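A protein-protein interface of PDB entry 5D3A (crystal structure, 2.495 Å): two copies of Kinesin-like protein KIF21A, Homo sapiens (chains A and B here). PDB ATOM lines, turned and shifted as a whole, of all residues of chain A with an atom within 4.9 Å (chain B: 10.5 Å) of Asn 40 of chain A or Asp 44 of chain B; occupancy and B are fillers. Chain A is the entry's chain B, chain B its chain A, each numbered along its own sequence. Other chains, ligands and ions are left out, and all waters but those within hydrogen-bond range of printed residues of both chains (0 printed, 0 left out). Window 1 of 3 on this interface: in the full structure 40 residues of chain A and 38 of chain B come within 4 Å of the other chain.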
ATOM      1  N   LYS A  35     -15.664  25.675  29.038  1.00  0.00           N
ATOM      2  CA  LYS A  35     -14.604  25.147  28.189  1.00  0.00           C
ATOM      3  C   LYS A  35     -15.103  23.950  27.387  1.00  0.00           C
ATOM      4  O   LYS A  35     -15.156  23.991  26.159  1.00  0.00           O
ATOM      5  CB  LYS A  35     -13.393  24.747  29.032  1.00  0.00           C
ATOM      6  CG  LYS A  35     -12.690  25.921  29.700  1.00  0.00           C
ATOM      7  CD  LYS A  35     -11.528  25.460  30.572  1.00  0.00           C
ATOM      8  CE  LYS A  35     -10.881  26.627  31.308  1.00  0.00           C
ATOM      9  NZ  LYS A  35      -9.777  26.183  32.205  1.00  0.00           N
ATOM     10  N   ILE A  36     -15.482  22.891  28.096  1.00  0.00           N
ATOM     11  CA  ILE A  36     -15.906  21.648  27.462  1.00  0.00           C
ATOM     12  C   ILE A  36     -17.016  21.912  26.450  1.00  0.00           C
ATOM     13  O   ILE A  36     -17.116  21.229  25.432  1.00  0.00           O
ATOM     14  CB  ILE A  36     -16.366  20.619  28.513  1.00  0.00           C
ATOM     15  CG1 ILE A  36     -15.244  20.341  29.515  1.00  0.00           C
ATOM     16  CG2 ILE A  36     -16.791  19.319  27.839  1.00  0.00           C
ATOM     17  CD1 ILE A  36     -15.692  19.567  30.728  1.00  0.00           C
ATOM     18  N   VAL A  37     -17.851  22.904  26.735  1.00  0.00           N
ATOM     19  CA  VAL A  37     -18.958  23.242  25.851  1.00  0.00           C
ATOM     20  C   VAL A  37     -18.433  23.937  24.596  1.00  0.00           C
ATOM     21  O   VAL A  37     -18.583  23.421  23.488  1.00  0.00           O
ATOM     22  CB  VAL A  37     -19.998  24.115  26.585  1.00  0.00           C
ATOM     23  CG1 VAL A  37     -20.997  24.725  25.610  1.00  0.00           C
ATOM     24  CG2 VAL A  37     -20.719  23.294  27.640  1.00  0.00           C
ATOM     25  N   LYS A  38     -17.816  25.102  24.772  1.00  0.00           N
ATOM     26  CA  LYS A  38     -17.301  25.877  23.647  1.00  0.00           C
ATOM     27  C   LYS A  38     -16.444  25.012  22.729  1.00  0.00           C
ATOM     28  O   LYS A  38     -16.526  25.124  21.505  1.00  0.00           O
ATOM     29  CB  LYS A  38     -16.497  27.078  24.150  1.00  0.00           C
ATOM     30  CG  LYS A  38     -17.359  28.211  24.694  1.00  0.00           C
ATOM     31  CD  LYS A  38     -16.546  29.207  25.511  1.00  0.00           C
ATOM     32  CE  LYS A  38     -15.508  29.930  24.668  1.00  0.00           C
ATOM     33  NZ  LYS A  38     -14.717  30.898  25.480  1.00  0.00           N
ATOM     34  N   GLU A  39     -15.628  24.146  23.324  1.00  0.00           N
ATOM     35  CA  GLU A  39     -14.824  23.201  22.556  1.00  0.00           C
ATOM     36  C   GLU A  39     -15.720  22.354  21.656  1.00  0.00           C
ATOM     37  O   GLU A  39     -15.402  22.122  20.489  1.00  0.00           O
ATOM     38  CB  GLU A  39     -14.007  22.304  23.487  1.00  0.00           C
ATOM     39  CG  GLU A  39     -12.875  23.026  24.206  1.00  0.00           C
ATOM     40  CD  GLU A  39     -12.102  22.117  25.143  1.00  0.00           C
ATOM     41  OE1 GLU A  39     -12.513  20.950  25.315  1.00  0.00           O
ATOM     42  OE2 GLU A  39     -11.083  22.570  25.707  1.00  0.00           O
ATOM     43  N   ASN A  40     -16.843  21.896  22.204  1.00  0.00           N
ATOM     44  CA  ASN A  40     -17.818  21.142  21.422  1.00  0.00           C
ATOM     45  C   ASN A  40     -18.461  22.040  20.368  1.00  0.00           C
ATOM     46  O   ASN A  40     -18.873  21.566  19.309  1.00  0.00           O
ATOM     47  CB  ASN A  40     -18.899  20.543  22.327  1.00  0.00           C
ATOM     48  CG  ASN A  40     -18.351  19.505  23.282  1.00  0.00           C
ATOM     49  OD1 ASN A  40     -17.148  19.450  23.538  1.00  0.00           O
ATOM     50  ND2 ASN A  40     -19.233  18.671  23.814  1.00  0.00           N
ATOM     51  N   GLY A  41     -18.543  23.333  20.668  1.00  0.00           N
ATOM     52  CA  GLY A  41     -19.131  24.299  19.758  1.00  0.00           C
ATOM     53  C   GLY A  41     -18.449  24.312  18.405  1.00  0.00           C
ATOM     54  O   GLY A  41     -19.098  24.474  17.370  1.00  0.00           O
ATOM     55  N   GLU A  42     -17.131  24.147  18.416  1.00  0.00           N
ATOM     56  CA  GLU A  42     -16.367  24.018  17.183  1.00  0.00           C
ATOM     57  C   GLU A  42     -16.568  22.625  16.589  1.00  0.00           C
ATOM     58  O   GLU A  42     -16.511  22.445  15.372  1.00  0.00           O
ATOM     59  CB  GLU A  42     -14.882  24.286  17.436  1.00  0.00           C
ATOM     60  CG  GLU A  42     -14.484  25.747  17.295  1.00  0.00           C
ATOM     61  CD  GLU A  42     -14.526  26.225  15.852  1.00  0.00           C
ATOM     62  OE1 GLU A  42     -14.389  25.382  14.938  1.00  0.00           O
ATOM     63  OE2 GLU A  42     -14.699  27.443  15.633  1.00  0.00           O
ATOM     64  N   GLY A  43     -16.804  21.646  17.455  1.00  0.00           N
ATOM     65  CA  GLY A  43     -17.070  20.291  17.012  1.00  0.00           C
ATOM     66  C   GLY A  43     -18.289  20.231  16.115  1.00  0.00           C
ATOM     67  O   GLY A  43     -18.239  19.665  15.025  1.00  0.00           O
ATOM     68  N   ASP A  44     -19.387  20.826  16.569  1.00  0.00           N
ATOM     69  CA  ASP A  44     -20.614  20.861  15.782  1.00  0.00           C
ATOM     70  C   ASP A  44     -20.400  21.611  14.473  1.00  0.00           C
ATOM     71  O   ASP A  44     -20.969  21.249  13.444  1.00  0.00           O
ATOM     72  CB  ASP A  44     -21.747  21.511  16.576  1.00  0.00           C
ATOM     73  CG  ASP A  44     -22.206  20.656  17.737  1.00  0.00           C
ATOM     74  OD1 ASP A  44     -22.235  19.416  17.587  1.00  0.00           O
ATOM     75  OD2 ASP A  44     -22.535  21.223  18.801  1.00  0.00           O
ATOM     76  N   LYS B  35     -15.034  10.628  14.457  1.00  0.00           N
ATOM     77  CA  LYS B  35     -14.030  10.959  15.458  1.00  0.00           C
ATOM     78  C   LYS B  35     -14.515  12.129  16.308  1.00  0.00           C
ATOM     79  O   LYS B  35     -14.347  12.138  17.527  1.00  0.00           O
ATOM     80  CB  LYS B  35     -12.695  11.301  14.793  1.00  0.00           C
ATOM     81  CG  LYS B  35     -11.538  11.513  15.768  1.00  0.00           C
ATOM     82  CD  LYS B  35     -11.242  10.254  16.575  1.00  0.00           C
ATOM     83  CE  LYS B  35      -9.979  10.399  17.414  1.00  0.00           C
ATOM     84  NZ  LYS B  35     -10.076  11.510  18.400  1.00  0.00           N
ATOM     85  N   ILE B  36     -15.128  13.109  15.653  1.00  0.00           N
ATOM     86  CA  ILE B  36     -15.604  14.310  16.328  1.00  0.00           C
ATOM     87  C   ILE B  36     -16.793  13.974  17.224  1.00  0.00           C
ATOM     88  O   ILE B  36     -16.934  14.520  18.318  1.00  0.00           O
ATOM     89  CB  ILE B  36     -15.973  15.402  15.308  1.00  0.00           C
ATOM     90  CG1 ILE B  36     -14.763  15.730  14.426  1.00  0.00           C
ATOM     91  CG2 ILE B  36     -16.474  16.656  16.021  1.00  0.00           C
ATOM     92  CD1 ILE B  36     -15.081  16.627  13.248  1.00  0.00           C
ATOM     93  N   VAL B  37     -17.647  13.075  16.751  1.00  0.00           N
ATOM     94  CA  VAL B  37     -18.802  12.631  17.522  1.00  0.00           C
ATOM     95  C   VAL B  37     -18.339  12.001  18.829  1.00  0.00           C
ATOM     96  O   VAL B  37     -19.035  12.075  19.841  1.00  0.00           O
ATOM     97  CB  VAL B  37     -19.664  11.646  16.704  1.00  0.00           C
ATOM     98  CG1 VAL B  37     -20.654  10.902  17.598  1.00  0.00           C
ATOM     99  CG2 VAL B  37     -20.391  12.386  15.597  1.00  0.00           C
ATOM    100  N   LYS B  38     -17.165  11.379  18.804  1.00  0.00           N
ATOM    101  CA  LYS B  38     -16.615  10.746  19.997  1.00  0.00           C
ATOM    102  C   LYS B  38     -16.029  11.798  20.932  1.00  0.00           C
ATOM    103  O   LYS B  38     -16.232  11.741  22.144  1.00  0.00           O
ATOM    104  CB  LYS B  38     -15.549   9.713  19.622  1.00  0.00           C
ATOM    105  CG  LYS B  38     -16.103   8.486  18.913  1.00  0.00           C
ATOM    106  CD  LYS B  38     -15.005   7.486  18.589  1.00  0.00           C
ATOM    107  CE  LYS B  38     -15.531   6.346  17.732  1.00  0.00           C
ATOM    108  NZ  LYS B  38     -16.713   5.679  18.347  1.00  0.00           N
ATOM    109  N   GLU B  39     -15.305  12.756  20.361  1.00  0.00           N
ATOM    110  CA  GLU B  39     -14.737  13.850  21.139  1.00  0.00           C
ATOM    111  C   GLU B  39     -15.832  14.605  21.886  1.00  0.00           C
ATOM    112  O   GLU B  39     -15.822  14.674  23.115  1.00  0.00           O
ATOM    113  CB  GLU B  39     -13.960  14.806  20.231  1.00  0.00           C
ATOM    114  CG  GLU B  39     -12.678  14.217  19.667  1.00  0.00           C
ATOM    115  CD  GLU B  39     -11.935  15.189  18.771  1.00  0.00           C
ATOM    116  OE1 GLU B  39     -12.526  16.229  18.402  1.00  0.00           O
ATOM    117  OE2 GLU B  39     -10.761  14.916  18.439  1.00  0.00           O
ATOM    118  N   ASN B  40     -16.778  15.167  21.140  1.00  0.00           N
ATOM    119  CA  ASN B  40     -17.890  15.897  21.740  1.00  0.00           C
ATOM    120  C   ASN B  40     -18.644  15.027  22.740  1.00  0.00           C
ATOM    121  O   ASN B  40     -19.107  15.514  23.772  1.00  0.00           O
ATOM    122  CB  ASN B  40     -18.851  16.394  20.660  1.00  0.00           C
ATOM    123  CG  ASN B  40     -18.248  17.483  19.800  1.00  0.00           C
ATOM    124  OD1 ASN B  40     -17.026  17.613  19.703  1.00  0.00           O
ATOM    125  ND2 ASN B  40     -19.106  18.276  19.169  1.00  0.00           N
ATOM    126  N   GLY B  41     -18.766  13.741  22.426  1.00  0.00           N
ATOM    127  CA  GLY B  41     -19.464  12.803  23.287  1.00  0.00           C
ATOM    128  C   GLY B  41     -18.854  12.692  24.671  1.00  0.00           C
ATOM    129  O   GLY B  41     -19.547  12.854  25.675  1.00  0.00           O
ATOM    130  N   GLU B  42     -17.554  12.412  24.726  1.00  0.00           N
ATOM    131  CA  GLU B  42     -16.848  12.285  25.998  1.00  0.00           C
ATOM    132  C   GLU B  42     -16.973  13.569  26.821  1.00  0.00           C
ATOM    133  O   GLU B  42     -17.217  13.523  28.027  1.00  0.00           O
ATOM    134  CB  GLU B  42     -15.371  11.951  25.760  1.00  0.00           C
ATOM    135  CG  GLU B  42     -14.578  11.666  27.033  1.00  0.00           C
ATOM    136  CD  GLU B  42     -13.092  11.489  26.772  1.00  0.00           C
ATOM    137  OE1 GLU B  42     -12.321  11.374  27.750  1.00  0.00           O
ATOM    138  OE2 GLU B  42     -12.696  11.466  25.588  1.00  0.00           O
ATOM    139  N   GLY B  43     -16.804  14.712  26.164  1.00  0.00           N
ATOM    140  CA  GLY B  43     -16.903  15.994  26.836  1.00  0.00           C
ATOM    141  C   GLY B  43     -18.272  16.214  27.450  1.00  0.00           C
ATOM    142  O   GLY B  43     -18.388  16.648  28.596  1.00  0.00           O
ATOM    143  N   ASP B  44     -19.312  15.904  26.685  1.00  0.00           N
ATOM    144  CA  ASP B  44     -20.682  16.072  27.155  1.00  0.00           C
ATOM    145  C   ASP B  44     -20.996  15.126  28.311  1.00  0.00           C
ATOM    146  O   ASP B  44     -22.028  15.267  28.969  1.00  0.00           O
ATOM    147  CB  ASP B  44     -21.668  15.848  26.009  1.00  0.00           C
ATOM    148  CG  ASP B  44     -21.563  16.915  24.934  1.00  0.00           C
ATOM    149  OD1 ASP B  44     -21.432  18.110  25.282  1.00  0.00           O
ATOM    150  OD2 ASP B  44     -21.608  16.557  23.738  1.00  0.00           O
ATOM    151  N   LYS B  45     -20.115  14.158  28.551  1.00  0.00           N
ATOM    152  CA  LYS B  45     -20.247  13.284  29.713  1.00  0.00           C
ATOM    153  C   LYS B  45     -19.633  13.967  30.927  1.00  0.00           C
ATOM    154  O   LYS B  45     -20.181  13.899  32.028  1.00  0.00           O
ATOM    155  CB  LYS B  45     -19.577  11.930  29.466  1.00  0.00           C
ATOM    156  CG  LYS B  45     -20.274  11.075  28.419  1.00  0.00           C
ATOM    157  CD  LYS B  45     -19.509   9.786  28.156  1.00  0.00           C
ATOM    158  CE  LYS B  45     -20.174   8.953  27.072  1.00  0.00           C
ATOM    159  NZ  LYS B  45     -19.402   7.716  26.766  1.00  0.00           N
ATOM    160  N   ASN B  46     -18.495  14.622  30.723  1.00  0.00           N
ATOM    161  CA  ASN B  46     -17.891  15.436  31.770  1.00  0.00           C
ATOM    162  C   ASN B  46     -18.893  16.485  32.235  1.00  0.00           C
ATOM    163  O   ASN B  46     -19.134  16.640  33.431  1.00  0.00           O
ATOM    164  CB  ASN B  46     -16.610  16.112  31.272  1.00  0.00           C
ATOM    165  CG  ASN B  46     -15.499  15.125  30.996  1.00  0.00           C
ATOM    166  OD1 ASN B  46     -14.953  15.079  29.894  1.00  0.00           O
ATOM    167  ND2 ASN B  46     -15.155  14.329  31.999  1.00  0.00           N
ATOM    168  N   VAL B  47     -19.475  17.197  31.275  1.00  0.00           N
ATOM    169  CA  VAL B  47     -20.449  18.240  31.564  1.00  0.00           C
ATOM    170  C   VAL B  47     -21.573  17.685  32.435  1.00  0.00           C
ATOM    171  O   VAL B  47     -21.971  18.307  33.421  1.00  0.00           O
ATOM    172  CB  VAL B  47     -21.009  18.845  30.261  1.00  0.00           C
ATOM    173  CG1 VAL B  47     -22.135  19.820  30.558  1.00  0.00           C
ATOM    174  CG2 VAL B  47     -19.904  19.535  29.482  1.00  0.00           C
ATOM    175  N   ALA B  48     -22.080  16.515  32.067  1.00  0.00           N
ATOM    176  CA  ALA B  48     -23.152  15.874  32.818  1.00  0.00           C
ATOM    177  C   ALA B  48     -22.759  15.712  34.279  1.00  0.00           C
ATOM    178  O   ALA B  48     -23.572  15.918  35.178  1.00  0.00           O
ATOM    179  CB  ALA B  48     -23.490  14.526  32.209  1.00  0.00           C
ATOM    180  N   ASN B  49     -21.503  15.340  34.506  1.00  0.00           N
ATOM    181  CA  ASN B  49     -20.983  15.162  35.856  1.00  0.00           C
ATOM    182  C   ASN B  49     -20.790  16.508  36.545  1.00  0.00           C
ATOM    183  O   ASN B  49     -21.087  16.653  37.729  1.00  0.00           O
ATOM    184  CB  ASN B  49     -19.662  14.391  35.822  1.00  0.00           C
ATOM    185  CG  ASN B  49     -19.850  12.921  35.494  1.00  0.00           C
ATOM    186  OD1 ASN B  49     -20.921  12.500  35.060  1.00  0.00           O
ATOM    187  ND2 ASN B  49     -18.802  12.131  35.702  1.00  0.00           N
ATOM    188  N   ILE B  50     -20.285  17.488  35.801  1.00  0.00           N
ATOM    189  CA  ILE B  50     -20.123  18.837  36.325  1.00  0.00           C
ATOM    190  C   ILE B  50     -21.473  19.335  36.820  1.00  0.00           C
ATOM    191  O   ILE B  50     -21.569  19.945  37.886  1.00  0.00           O
ATOM    192  CB  ILE B  50     -19.530  19.785  35.265  1.00  0.00           C
ATOM    193  CG1 ILE B  50     -18.086  19.384  34.955  1.00  0.00           C
ATOM    194  CG2 ILE B  50     -19.571  21.229  35.746  1.00  0.00           C
ATOM    195  CD1 ILE B  50     -17.460  20.147  33.799  1.00  0.00           C
ATOM    196  N   ASN B  51     -22.515  19.069  36.041  1.00  0.00           N
ATOM    197  CA  ASN B  51     -23.861  19.491  36.404  1.00  0.00           C
ATOM    198  C   ASN B  51     -24.296  18.862  37.720  1.00  0.00           C
ATOM    199  O   ASN B  51     -24.720  19.559  38.640  1.00  0.00           O
ATOM    200  CB  ASN B  51     -24.850  19.130  35.298  1.00  0.00           C
ATOM    201  CG  ASN B  51     -24.706  20.019  34.081  1.00  0.00           C
ATOM    202  OD1 ASN B  51     -24.101  21.090  34.145  1.00  0.00           O
ATOM    203  ND2 ASN B  51     -25.272  19.582  32.964  1.00  0.00           N
ATOM    204  N   GLU B  52     -24.181  17.542  37.808  1.00  0.00           N
ATOM    205  CA  GLU B  52     -24.567  16.820  39.015  1.00  0.00           C
ATOM    206  C   GLU B  52     -23.834  17.374  40.235  1.00  0.00           C
ATOM    207  O   GLU B  52     -24.372  17.393  41.344  1.00  0.00           O
ATOM    208  CB  GLU B  52     -24.282  15.325  38.854  1.00  0.00           C
ATOM    209  CG  GLU B  52     -25.109  14.657  37.768  1.00  0.00           C
ATOM    210  CD  GLU B  52     -24.704  13.218  37.515  1.00  0.00           C
ATOM    211  OE1 GLU B  52     -23.792  12.719  38.206  1.00  0.00           O
ATOM    212  OE2 GLU B  52     -25.301  12.585  36.620  1.00  0.00           O
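The backbone carbonyl oxygen (O) of Asn 40 of chain B lies within hydrogen-bond range of the side-chain amide nitrogen (ND2) of Asn 40 of chain A (3.2 Å).
ND2 of Asn 40 of chain A lies within hydrogen-bond range of OD1 of Asp 44 of chain B (2.7 Å).
The backbone carbonyl oxygen of Ile 36 of chain B lies close to the side-chain amide oxygen of Asn 40 of chain B, at 3.4 Å.
The side-chain carboxylate (OD2) of Asp 44 of chain B sits close to the backbone carbonyl oxygen (O) of Asn 40 of chain B.
O of Glu 42 of chain B sits close to OD1 of Asn 46 of chain B.
The backbone carbonyl oxygen (O) of Ile 36 of chain A lies close to the side-chain amide oxygen (OD1) of Asn 40 of chain A (2.6 Å).
Among the printed residues, merely in contact across the chains: Ile 36 of chain A with Gly 43 of chain B, Ile 36 of chain A with Asn 46 of chain B, Ile 36 of chain A with Val 47 of chain B, Ile 36 of chain A with Ile 50 of chain B, Gly 43 of chain A with Ile 36 of chain B, Gly 43 of chain A with Asn 40 of chain B and Asp 44 of chain A with Asn 40 of chain B.
Asn 40 of chain A touches two residues of chain B.
Of chain A, only Asn 40 (2.7 Å) comes within 4 Å of Asp 44 of chain B.
No residue of chain B comes within 4 Å of Val 37 of chain A.
Printed residues of chain B within 4 Å of Gly 43 of chain A: Ile 36 (3.6 Å) and Asn 40 (3.6 Å).
Asp 44 of chain A touches just one residue of chain B: Asn 40 (3.7 Å).
Of the printed residues of chain B, Ile 36 of chain A touches Gly 43 (3.2 Å), Asn 46 (3.6 Å), Val 47 (3.5 Å) and Ile 50 (3.6 Å).
Printed residues of chain A within 4 Å of Asn 46 of chain B: Ile 36.
Glu 39 of chain A touches none of the printed residues of chain B.
Asn 51 of chain B touches none of the printed residues of chain A.
The nearest printed residue of chain A that does not touch Asn 46 of chain B is Glu 39 of chain A (7.8 Å).
Of the 18 printed residues of chain B, 7 touch a printed residue of chain A.
Along chain B the printed residues that touch a printed residue of chain A span positions 36 to 50.
Hydrophobic or aromatic side chains of chain A that line the printed part of chain B: Ile 36.
Among the printed residues, no Asp or Glu carboxylate lies within 4 Å of a Lys or Arg side-chain nitrogen of the other chain.
Ile 36 of chain A touches Gly 43 of chain B, and with the chains exchanged Gly 43 of chain A touches Ile 36 of chain B.
Asn 40 of chain B touches its own counterpart, Asn 40 of chain A.
Asn 40 of chain A touches Asp 44 of chain B, and with the chains exchanged Asp 44 of chain A touches Asn 40 of chain B.
Gly 43 of chain A touches Asn 40 of chain B, but with the chains exchanged Asn 40 of chain A does not touch Gly 43 of chain B (4.5 Å).
Positions printed for both chains: 35, 36, 37, 38, 39, 40, 41, 42, 43 and 44.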
